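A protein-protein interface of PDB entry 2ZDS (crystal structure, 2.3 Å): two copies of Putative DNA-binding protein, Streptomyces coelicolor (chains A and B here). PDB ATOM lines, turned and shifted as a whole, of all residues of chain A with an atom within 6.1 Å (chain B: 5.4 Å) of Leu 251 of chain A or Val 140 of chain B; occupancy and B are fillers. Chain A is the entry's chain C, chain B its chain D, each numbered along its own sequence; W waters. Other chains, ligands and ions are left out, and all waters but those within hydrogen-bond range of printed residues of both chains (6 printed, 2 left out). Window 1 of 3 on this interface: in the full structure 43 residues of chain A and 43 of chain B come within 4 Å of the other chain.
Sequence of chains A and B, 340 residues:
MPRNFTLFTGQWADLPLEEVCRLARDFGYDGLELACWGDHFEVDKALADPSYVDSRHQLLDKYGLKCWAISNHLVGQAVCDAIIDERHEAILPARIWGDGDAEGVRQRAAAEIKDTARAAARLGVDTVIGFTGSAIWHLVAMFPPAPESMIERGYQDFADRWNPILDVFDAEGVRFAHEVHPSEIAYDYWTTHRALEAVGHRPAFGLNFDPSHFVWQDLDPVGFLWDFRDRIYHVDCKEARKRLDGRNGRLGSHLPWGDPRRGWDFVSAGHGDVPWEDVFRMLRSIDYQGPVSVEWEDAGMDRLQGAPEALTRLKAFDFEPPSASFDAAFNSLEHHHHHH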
ATOM      1  N   TRP A 137      33.275  12.285 -34.443  1.00  0.00           N
ATOM      2  CA  TRP A 137      32.626  12.744 -33.208  1.00  0.00           C
ATOM      3  C   TRP A 137      32.245  11.600 -32.286  1.00  0.00           C
ATOM      4  O   TRP A 137      32.428  11.704 -31.054  1.00  0.00           O
ATOM      5  CB  TRP A 137      31.389  13.617 -33.484  1.00  0.00           C
ATOM      6  CG  TRP A 137      30.565  13.873 -32.178  1.00  0.00           C
ATOM      7  CD1 TRP A 137      29.366  13.286 -31.818  1.00  0.00           C
ATOM      8  CD2 TRP A 137      30.943  14.712 -31.072  1.00  0.00           C
ATOM      9  NE1 TRP A 137      28.977  13.734 -30.571  1.00  0.00           N
ATOM     10  CE2 TRP A 137      29.923  14.605 -30.095  1.00  0.00           C
ATOM     11  CE3 TRP A 137      32.051  15.541 -30.811  1.00  0.00           C
ATOM     12  CZ2 TRP A 137      29.980  15.307 -28.875  1.00  0.00           C
ATOM     13  CZ3 TRP A 137      32.110  16.238 -29.601  1.00  0.00           C
ATOM     14  CH2 TRP A 137      31.080  16.120 -28.654  1.00  0.00           C
ATOM     15  N   VAL A 140      34.457  10.289 -29.447  1.00  0.00           N
ATOM     16  CA  VAL A 140      34.850  11.292 -28.429  1.00  0.00           C
ATOM     17  C   VAL A 140      35.240  10.672 -27.071  1.00  0.00           C
ATOM     18  O   VAL A 140      36.249  11.089 -26.444  1.00  0.00           O
ATOM     19  CB  VAL A 140      33.767  12.446 -28.277  1.00  0.00           C
ATOM     20  CG1 VAL A 140      32.424  11.959 -27.615  1.00  0.00           C
ATOM     21  CG2 VAL A 140      34.363  13.623 -27.533  1.00  0.00           C
ATOM     22  N   TRP A 216      29.454  24.275 -20.401  1.00  0.00           N
ATOM     23  CA  TRP A 216      29.640  22.952 -19.782  1.00  0.00           C
ATOM     24  C   TRP A 216      30.993  22.302 -20.035  1.00  0.00           C
ATOM     25  O   TRP A 216      31.392  21.382 -19.297  1.00  0.00           O
ATOM     26  CB  TRP A 216      28.539  21.992 -20.212  1.00  0.00           C
ATOM     27  CG  TRP A 216      28.559  21.509 -21.643  1.00  0.00           C
ATOM     28  CD1 TRP A 216      27.953  22.098 -22.718  1.00  0.00           C
ATOM     29  CD2 TRP A 216      29.180  20.316 -22.139  1.00  0.00           C
ATOM     30  NE1 TRP A 216      28.161  21.343 -23.858  1.00  0.00           N
ATOM     31  CE2 TRP A 216      28.909  20.246 -23.532  1.00  0.00           C
ATOM     32  CE3 TRP A 216      29.947  19.295 -21.547  1.00  0.00           C
ATOM     33  CZ2 TRP A 216      29.365  19.186 -24.338  1.00  0.00           C
ATOM     34  CZ3 TRP A 216      30.413  18.241 -22.363  1.00  0.00           C
ATOM     35  CH2 TRP A 216      30.081  18.186 -23.731  1.00  0.00           C
ATOM     36  N   GLY A 249      24.840  15.513 -14.258  1.00  0.00           N
ATOM     37  CA  GLY A 249      26.185  15.497 -14.820  1.00  0.00           C
ATOM     38  C   GLY A 249      26.424  16.452 -15.997  1.00  0.00           C
ATOM     39  O   GLY A 249      25.497  16.933 -16.619  1.00  0.00           O
ATOM     40  N   ARG A 250      27.684  16.708 -16.310  1.00  0.00           N
ATOM     41  CA  ARG A 250      28.061  17.603 -17.401  1.00  0.00           C
ATOM     42  C   ARG A 250      27.538  17.249 -18.796  1.00  0.00           C
ATOM     43  O   ARG A 250      27.440  18.142 -19.656  1.00  0.00           O
ATOM     44  CB  ARG A 250      29.587  17.717 -17.436  1.00  0.00           C
ATOM     45  CG  ARG A 250      30.131  18.424 -16.198  1.00  0.00           C
ATOM     46  CD  ARG A 250      30.719  19.719 -16.556  1.00  0.00           C
ATOM     47  NE  ARG A 250      31.096  20.503 -15.406  1.00  0.00           N
ATOM     48  CZ  ARG A 250      31.415  21.787 -15.492  1.00  0.00           C
ATOM     49  NH1 ARG A 250      31.417  22.359 -16.688  1.00  0.00           N
ATOM     50  NH2 ARG A 250      31.689  22.503 -14.399  1.00  0.00           N
ATOM     51  N   LEU A 251      27.252  15.961 -19.022  1.00  0.00           N
ATOM     52  CA  LEU A 251      26.792  15.433 -20.313  1.00  0.00           C
ATOM     53  C   LEU A 251      25.270  15.505 -20.464  1.00  0.00           C
ATOM     54  O   LEU A 251      24.764  15.385 -21.572  1.00  0.00           O
ATOM     55  CB  LEU A 251      27.249  13.985 -20.500  1.00  0.00           C
ATOM     56  CG  LEU A 251      28.709  13.684 -20.840  1.00  0.00           C
ATOM     57  CD1 LEU A 251      28.975  12.164 -20.754  1.00  0.00           C
ATOM     58  CD2 LEU A 251      29.091  14.296 -22.224  1.00  0.00           C
ATOM     59  N   GLY A 252      24.532  15.721 -19.378  1.00  0.00           N
ATOM     60  CA  GLY A 252      23.090  15.912 -19.522  1.00  0.00           C
ATOM     61  C   GLY A 252      22.239  14.643 -19.456  1.00  0.00           C
ATOM     62  O   GLY A 252      21.023  14.734 -19.387  1.00  0.00           O
ATOM     63  N   SER A 253      22.890  13.461 -19.446  1.00  0.00           N
ATOM     64  CA  SER A 253      22.231  12.169 -19.209  1.00  0.00           C
ATOM     65  C   SER A 253      21.240  11.722 -20.317  1.00  0.00           C
ATOM     66  O   SER A 253      20.337  10.937 -20.046  1.00  0.00           O
ATOM     67  CB  SER A 253      21.611  12.075 -17.795  1.00  0.00           C
ATOM     68  OG  SER A 253      22.482  12.652 -16.838  1.00  0.00           O
ATOM     69  N   HIS A 254      21.426  12.198 -21.561  1.00  0.00           N
ATOM     70  CA  HIS A 254      20.441  11.917 -22.645  1.00  0.00           C
ATOM     71  C   HIS A 254      19.019  12.424 -22.331  1.00  0.00           C
ATOM     72  O   HIS A 254      18.039  11.949 -22.900  1.00  0.00           O
ATOM     73  CB  HIS A 254      20.406  10.414 -23.012  1.00  0.00           C
ATOM     74  CG  HIS A 254      21.624   9.926 -23.756  1.00  0.00           C
ATOM     75  ND1 HIS A 254      22.842   9.709 -23.144  1.00  0.00           N
ATOM     76  CD2 HIS A 254      21.802   9.594 -25.061  1.00  0.00           C
ATOM     77  CE1 HIS A 254      23.708   9.238 -24.026  1.00  0.00           C
ATOM     78  NE2 HIS A 254      23.094   9.140 -25.193  1.00  0.00           N
ATOM     79  N   ARG A 262      19.300  17.538 -15.829  1.00  0.00           N
ATOM     80  CA  ARG A 262      20.408  17.892 -16.707  1.00  0.00           C
ATOM     81  C   ARG A 262      21.438  18.723 -15.933  1.00  0.00           C
ATOM     82  O   ARG A 262      21.034  19.658 -15.229  1.00  0.00           O
ATOM     83  CB  ARG A 262      19.894  18.813 -17.799  1.00  0.00           C
ATOM     84  CG  ARG A 262      19.018  18.216 -18.937  1.00  0.00           C
ATOM     85  CD  ARG A 262      19.171  19.205 -20.142  1.00  0.00           C
ATOM     86  NE  ARG A 262      19.517  18.294 -21.166  1.00  0.00           N
ATOM     87  CZ  ARG A 262      20.690  18.104 -21.724  1.00  0.00           C
ATOM     88  NH1 ARG A 262      21.696  18.930 -21.550  1.00  0.00           N
ATOM     89  NH2 ARG A 262      20.781  17.057 -22.539  1.00  0.00           N
ATOM     90  N   GLY A 263      22.740  18.432 -16.066  1.00  0.00           N
ATOM     91  CA  GLY A 263      23.798  19.281 -15.421  1.00  0.00           C
ATOM     92  C   GLY A 263      23.862  20.693 -15.990  1.00  0.00           C
ATOM     93  O   GLY A 263      24.428  21.595 -15.381  1.00  0.00           O
ATOM     94  N   TRP A 264      23.269  20.892 -17.175  1.00  0.00           N
ATOM     95  CA  TRP A 264      23.262  22.196 -17.846  1.00  0.00           C
ATOM     96  C   TRP A 264      22.077  22.279 -18.836  1.00  0.00           C
ATOM     97  O   TRP A 264      21.600  21.257 -19.364  1.00  0.00           O
ATOM     98  CB  TRP A 264      24.615  22.492 -18.549  1.00  0.00           C
ATOM     99  CG  TRP A 264      24.828  21.759 -19.790  1.00  0.00           C
ATOM    100  CD1 TRP A 264      25.367  20.505 -19.922  1.00  0.00           C
ATOM    101  CD2 TRP A 264      24.448  22.176 -21.108  1.00  0.00           C
ATOM    102  NE1 TRP A 264      25.352  20.123 -21.253  1.00  0.00           N
ATOM    103  CE2 TRP A 264      24.790  21.121 -21.998  1.00  0.00           C
ATOM    104  CE3 TRP A 264      23.840  23.336 -21.627  1.00  0.00           C
ATOM    105  CZ2 TRP A 264      24.578  21.202 -23.405  1.00  0.00           C
ATOM    106  CZ3 TRP A 264      23.614  23.410 -23.024  1.00  0.00           C
ATOM    107  CH2 TRP A 264      23.973  22.339 -23.880  1.00  0.00           C
ATOM    108  N   ILE B 136      22.786   3.816 -27.710  1.00  0.00           N
ATOM    109  CA  ILE B 136      22.432   5.232 -27.814  1.00  0.00           C
ATOM    110  C   ILE B 136      23.532   6.206 -27.402  1.00  0.00           C
ATOM    111  O   ILE B 136      23.312   7.413 -27.447  1.00  0.00           O
ATOM    112  CB  ILE B 136      21.097   5.568 -27.055  1.00  0.00           C
ATOM    113  CG1 ILE B 136      21.189   5.197 -25.555  1.00  0.00           C
ATOM    114  CG2 ILE B 136      19.857   4.955 -27.765  1.00  0.00           C
ATOM    115  CD1 ILE B 136      20.188   5.966 -24.650  1.00  0.00           C
ATOM    116  N   TRP B 137      24.697   5.679 -27.014  1.00  0.00           N
ATOM    117  CA  TRP B 137      25.796   6.494 -26.510  1.00  0.00           C
ATOM    118  C   TRP B 137      26.180   7.587 -27.501  1.00  0.00           C
ATOM    119  O   TRP B 137      26.436   8.728 -27.117  1.00  0.00           O
ATOM    120  CB  TRP B 137      27.039   5.656 -26.122  1.00  0.00           C
ATOM    121  CG  TRP B 137      28.221   6.570 -25.959  1.00  0.00           C
ATOM    122  CD1 TRP B 137      29.266   6.745 -26.850  1.00  0.00           C
ATOM    123  CD2 TRP B 137      28.466   7.495 -24.867  1.00  0.00           C
ATOM    124  NE1 TRP B 137      30.134   7.697 -26.361  1.00  0.00           N
ATOM    125  CE2 TRP B 137      29.677   8.160 -25.147  1.00  0.00           C
ATOM    126  CE3 TRP B 137      27.792   7.792 -23.666  1.00  0.00           C
ATOM    127  CZ2 TRP B 137      30.222   9.127 -24.281  1.00  0.00           C
ATOM    128  CZ3 TRP B 137      28.352   8.734 -22.796  1.00  0.00           C
ATOM    129  CH2 TRP B 137      29.540   9.391 -23.118  1.00  0.00           C
ATOM    130  N   HIS B 138      26.242   7.230 -28.776  1.00  0.00           N
ATOM    131  CA  HIS B 138      26.675   8.152 -29.860  1.00  0.00           C
ATOM    132  C   HIS B 138      25.692   9.307 -30.033  1.00  0.00           C
ATOM    133  O   HIS B 138      25.984  10.271 -30.732  1.00  0.00           O
ATOM    134  CB  HIS B 138      26.853   7.366 -31.202  1.00  0.00           C
ATOM    135  CG  HIS B 138      25.590   6.701 -31.697  1.00  0.00           C
ATOM    136  ND1 HIS B 138      24.931   7.097 -32.846  1.00  0.00           N
ATOM    137  CD2 HIS B 138      24.866   5.675 -31.192  1.00  0.00           C
ATOM    138  CE1 HIS B 138      23.847   6.355 -33.015  1.00  0.00           C
ATOM    139  NE2 HIS B 138      23.791   5.480 -32.030  1.00  0.00           N
ATOM    140  N   LEU B 139      24.524   9.198 -29.394  1.00  0.00           N
ATOM    141  CA  LEU B 139      23.486  10.229 -29.439  1.00  0.00           C
ATOM    142  C   LEU B 139      23.632  11.249 -28.289  1.00  0.00           C
ATOM    143  O   LEU B 139      22.782  12.158 -28.184  1.00  0.00           O
ATOM    144  CB  LEU B 139      22.100   9.598 -29.382  1.00  0.00           C
ATOM    145  CG  LEU B 139      21.682   8.558 -30.446  1.00  0.00           C
ATOM    146  CD1 LEU B 139      20.239   7.994 -30.234  1.00  0.00           C
ATOM    147  CD2 LEU B 139      21.821   9.187 -31.822  1.00  0.00           C
ATOM    148  N   VAL B 140      24.708  11.119 -27.460  1.00  0.00           N
ATOM    149  CA  VAL B 140      24.908  11.925 -26.229  1.00  0.00           C
ATOM    150  C   VAL B 140      24.790  13.452 -26.433  1.00  0.00           C
ATOM    151  O   VAL B 140      24.166  14.160 -25.617  1.00  0.00           O
ATOM    152  CB  VAL B 140      26.245  11.530 -25.438  1.00  0.00           C
ATOM    153  CG1 VAL B 140      27.525  11.767 -26.266  1.00  0.00           C
ATOM    154  CG2 VAL B 140      26.312  12.246 -24.041  1.00  0.00           C
ATOM    155  N   ALA B 141      25.362  13.937 -27.539  1.00  0.00           N
ATOM    156  CA  ALA B 141      25.383  15.374 -27.868  1.00  0.00           C
ATOM    157  C   ALA B 141      24.010  15.904 -28.288  1.00  0.00           C
ATOM    158  O   ALA B 141      23.766  17.099 -28.181  1.00  0.00           O
ATOM    159  CB  ALA B 141      26.395  15.670 -28.935  1.00  0.00           C
ATOM    160  N   MET B 142      23.123  15.041 -28.779  1.00  0.00           N
ATOM    161  CA  MET B 142      21.758  15.490 -29.096  1.00  0.00           C
ATOM    162  C   MET B 142      21.631  16.533 -30.246  1.00  0.00           C
ATOM    163  O   MET B 142      20.681  17.316 -30.298  1.00  0.00           O
ATOM    164  CB  MET B 142      21.053  15.978 -27.830  1.00  0.00           C
ATOM    165  CG  MET B 142      20.657  14.831 -26.879  1.00  0.00           C
ATOM    166  SD  MET B 142      19.579  15.468 -25.348  1.00  0.00           S
ATOM    167  CE  MET B 142      18.213  16.651 -26.124  1.00  0.00           C
ATOM    168  N   TYR B 187      26.372   5.666 -17.553  1.00  0.00           N
ATOM    169  CA  TYR B 187      27.666   6.348 -17.592  1.00  0.00           C
ATOM    170  C   TYR B 187      27.681   7.481 -16.549  1.00  0.00           C
ATOM    171  O   TYR B 187      28.708   8.136 -16.332  1.00  0.00           O
ATOM    172  CB  TYR B 187      27.953   6.906 -19.013  1.00  0.00           C
ATOM    173  CG  TYR B 187      26.919   7.899 -19.546  1.00  0.00           C
ATOM    174  CD1 TYR B 187      26.917   9.250 -19.112  1.00  0.00           C
ATOM    175  CD2 TYR B 187      25.967   7.513 -20.477  1.00  0.00           C
ATOM    176  CE1 TYR B 187      25.978  10.176 -19.576  1.00  0.00           C
ATOM    177  CE2 TYR B 187      25.009   8.467 -20.978  1.00  0.00           C
ATOM    178  CZ  TYR B 187      25.044   9.789 -20.502  1.00  0.00           C
ATOM    179  OH  TYR B 187      24.173  10.711 -20.970  1.00  0.00           O
ATOM    180  N   ASP B 188      26.531   7.621 -15.896  1.00  0.00           N
ATOM    181  CA  ASP B 188      26.056   8.768 -15.108  1.00  0.00           C
ATOM    182  C   ASP B 188      25.351   8.304 -13.884  1.00  0.00           C
ATOM    183  O   ASP B 188      24.837   7.194 -13.889  1.00  0.00           O
ATOM    184  CB  ASP B 188      24.844   9.474 -15.875  1.00  0.00           C
ATOM    185  CG  ASP B 188      25.224  10.717 -16.225  1.00  0.00           C
ATOM    186  OD1 ASP B 188      26.440  10.772 -16.003  1.00  0.00           O
ATOM    187  OD2 ASP B 188      24.498  11.614 -16.628  1.00  0.00           O
ATOM    188  N   TRP B 216      35.651  14.223 -14.294  1.00  0.00           N
ATOM    189  CA  TRP B 216      35.346  15.181 -15.369  1.00  0.00           C
ATOM    190  C   TRP B 216      33.857  15.544 -15.543  1.00  0.00           C
ATOM    191  O   TRP B 216      33.545  16.647 -15.984  1.00  0.00           O
ATOM    192  CB  TRP B 216      35.977  14.774 -16.689  1.00  0.00           C
ATOM    193  CG  TRP B 216      35.306  13.647 -17.422  1.00  0.00           C
ATOM    194  CD1 TRP B 216      35.571  12.313 -17.313  1.00  0.00           C
ATOM    195  CD2 TRP B 216      34.283  13.773 -18.428  1.00  0.00           C
ATOM    196  NE1 TRP B 216      34.776  11.606 -18.171  1.00  0.00           N
ATOM    197  CE2 TRP B 216      33.980  12.470 -18.874  1.00  0.00           C
ATOM    198  CE3 TRP B 216      33.602  14.871 -19.007  1.00  0.00           C
ATOM    199  CZ2 TRP B 216      33.044  12.226 -19.879  1.00  0.00           C
ATOM    200  CZ3 TRP B 216      32.632  14.617 -19.984  1.00  0.00           C
ATOM    201  CH2 TRP B 216      32.390  13.311 -20.427  1.00  0.00           C
ATOM    202  N   GLN B 217      32.971  14.615 -15.177  1.00  0.00           N
ATOM    203  CA  GLN B 217      31.516  14.782 -15.256  1.00  0.00           C
ATOM    204  C   GLN B 217      30.866  15.562 -14.084  1.00  0.00           C
ATOM    205  O   GLN B 217      29.636  15.815 -14.125  1.00  0.00           O
ATOM    206  CB  GLN B 217      30.856  13.399 -15.349  1.00  0.00           C
ATOM    207  CG  GLN B 217      30.979  12.745 -16.688  1.00  0.00           C
ATOM    208  CD  GLN B 217      30.160  11.448 -16.765  1.00  0.00           C
ATOM    209  OE1 GLN B 217      30.596  10.370 -16.324  1.00  0.00           O
ATOM    210  NE2 GLN B 217      28.963  11.555 -17.308  1.00  0.00           N
ATOM    211  N   LEU B 251      35.925  17.493 -22.484  1.00  0.00           N
ATOM    212  CA  LEU B 251      35.854  16.342 -23.412  1.00  0.00           C
ATOM    213  C   LEU B 251      37.201  15.745 -23.786  1.00  0.00           C
ATOM    214  O   LEU B 251      37.248  14.580 -24.171  1.00  0.00           O
ATOM    215  CB  LEU B 251      35.055  16.651 -24.710  1.00  0.00           C
ATOM    216  CG  LEU B 251      33.560  16.756 -24.557  1.00  0.00           C
ATOM    217  CD1 LEU B 251      32.831  17.217 -25.831  1.00  0.00           C
ATOM    218  CD2 LEU B 251      32.965  15.415 -24.022  1.00  0.00           C
HETATM  219  O   HOH W   1      25.725  16.151 -24.182  1.00  0.00           O
HETATM  220  O   HOH W   2      38.302  13.175 -26.260  1.00  0.00           O
HETATM  221  O   HOH W   3      22.849  14.165 -22.950  1.00  0.00           O
HETATM  222  O   HOH W   4      32.477   7.962 -27.925  1.00  0.00           O
HETATM  223  O   HOH W   5      23.951  12.015 -13.737  1.00  0.00           O
HETATM  224  O   HOH W   6      35.954  12.204 -23.603  1.00  0.00           O
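OD1 of Asp 188 of chain B sits at hydrogen-bond distance from NE2 of Gln 217 of chain B, at 2.9 Å. The backbone carbonyl oxygen (O) of Arg 250 of chain A lies close to the indole nitrogen (NE1) of Trp 264 of chain A. The guanidinium group of Arg 262 of chain A lies within hydrogen-bond range of the backbone carbonyl oxygen of Trp 264 of chain A (3.2 Å). NH1 of Arg 250 of chain A sits at hydrogen-bond distance from O of Trp 216 of chain A, 2.8 Å away. The backbone carbonyl oxygen (O) of Tyr 187 of chain B sits close to the side-chain amide oxygen (OE1) of Gln 217 of chain B. The backbone carbonyl oxygen (O) of Gly 249 of chain A lies close to the backbone NH (N) of Gly 263 of chain A (3.2 Å).
Leu 251 of chain A touches just these residues of chain B: Trp 137, Val 140, Tyr 187, Trp 216 and Gln 217. Val 140 of chain B touches just these residues of chain A: Leu 251 (3.9 Å) and His 254 (3.4 Å). Of the printed residues of chain B, Gly 249 of chain A touches Gln 217. Of the printed residues of chain A, Trp 137 of chain B touches Leu 251 (3.7 Å) and His 254 (3.9 Å). Printed residues of chain A within 4 Å of Trp 216 of chain B: Arg 250 and Leu 251. Gly 263 of chain A touches none of the printed residues of chain B.
ND1 of His 254 of chain A is in hydrogen-bond range of OH of Tyr 187 of chain B. The side-chain hydroxyl of Ser 253 of chain A sits close to the side-chain carboxylate of Asp 188 of chain B, 2.3 Å away. The side-chain hydroxyl (OH) of Tyr 187 of chain B sits close to the backbone NH (N) of Ser 253 of chain A (3.4 Å). A ring nitrogen (NE2) of His 254 of chain A is in hydrogen-bond range of the backbone carbonyl oxygen (O) of Ile 136 of chain B, 2.8 Å away. NH2 of Arg 262 of chain A is in hydrogen-bond range of SD of Met 142 of chain B (3.4 Å). The backbone NH (N) of Arg 250 of chain A lies within hydrogen-bond range of the backbone carbonyl oxygen (O) of Gln 217 of chain B (3.1 Å). A ring nitrogen (NE2) of His 254 of chain A sits at hydrogen-bond distance from the backbone NH (N) of Val 140 of chain B (3.4 Å).
Among the printed residues, merely in contact across the chains: Trp 137 of chain A with Leu 251 of chain B (3.5 Å), Leu 251 of chain A with Gln 217 of chain B (3.5 Å), Gly 249 of chain A with Gln 217 of chain B (3.5 Å), Trp 216 of chain A with Leu 251 of chain B (3.6 Å), Trp 137 of chain A with Ala 141 of chain B (3.6 Å), Leu 251 of chain A with Trp 216 of chain B (3.6 Å), Leu 251 of chain A with Trp 137 of chain B (3.7 Å), Leu 251 of chain A with Tyr 187 of chain B (3.8 Å), His 254 of chain A with Leu 139 of chain B (3.8 Å), Arg 250 of chain A with Trp 216 of chain B (3.9 Å), His 254 of chain A with Trp 137 of chain B (3.9 Å) and Leu 251 of chain A with Val 140 of chain B (3.9 Å).
Trp 137 of chain A touches Leu 251 of chain B, and with the chains exchanged Leu 251 of chain A touches Trp 137 of chain B. Trp 216 of chain A touches Leu 251 of chain B, and with the chains exchanged Leu 251 of chain A touches Trp 216 of chain B. Leu 251 of chain A touches Val 140 of chain B, but with the chains exchanged Val 140 of chain A does not touch Leu 251 of chain B (4.2 Å). Of the 19 pairs that touch across the chains among the printed residues, 4 have their exchanged pair printed and touching as well.
Hydrophobic or aromatic side chains of chain A that line the printed part of chain B: Trp 137, Trp 216, Leu 251 and His 254. Hydrophobic or aromatic side chains of chain B within 4 Å of the printed part of chain A: Ile 136, Trp 137, Val 140, Ala 141, Met 142, Tyr 187, Trp 216 and Leu 251. Among the printed residues, 19 pairs touch across the chains. Among the printed residues, no Asp or Glu carboxylate lies within 4 Å of a Lys or Arg side-chain nitrogen of the other chain.
Water W3 lies within hydrogen-bond range of O of Leu 251 of chain A, N of His 254 of chain A and O of Val 140 of chain B. Water W2 bridges the backbone carbonyl oxygen (O) of Leu 251 of chain B (2.7 Å) and the backbone carbonyl oxygen (O) of Val 140 of chain A (2.9 Å). Water W6 bridges O of Leu 251 of chain B (2.8 Å) and O of Val 140 of chain A (3.1 Å). Water W4 lies within hydrogen-bond range of the indole nitrogen of Trp 137 of chain B (2.8 Å) and the backbone NH of Val 140 of chain A (3.4 Å). Water W1 bridges O of Leu 251 of chain A (2.9 Å) and O of Val 140 of chain B (2.9 Å). Water W5 lies within hydrogen-bond range of OD2 of Asp 188 of chain B and OG of Ser 253 of chain A.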
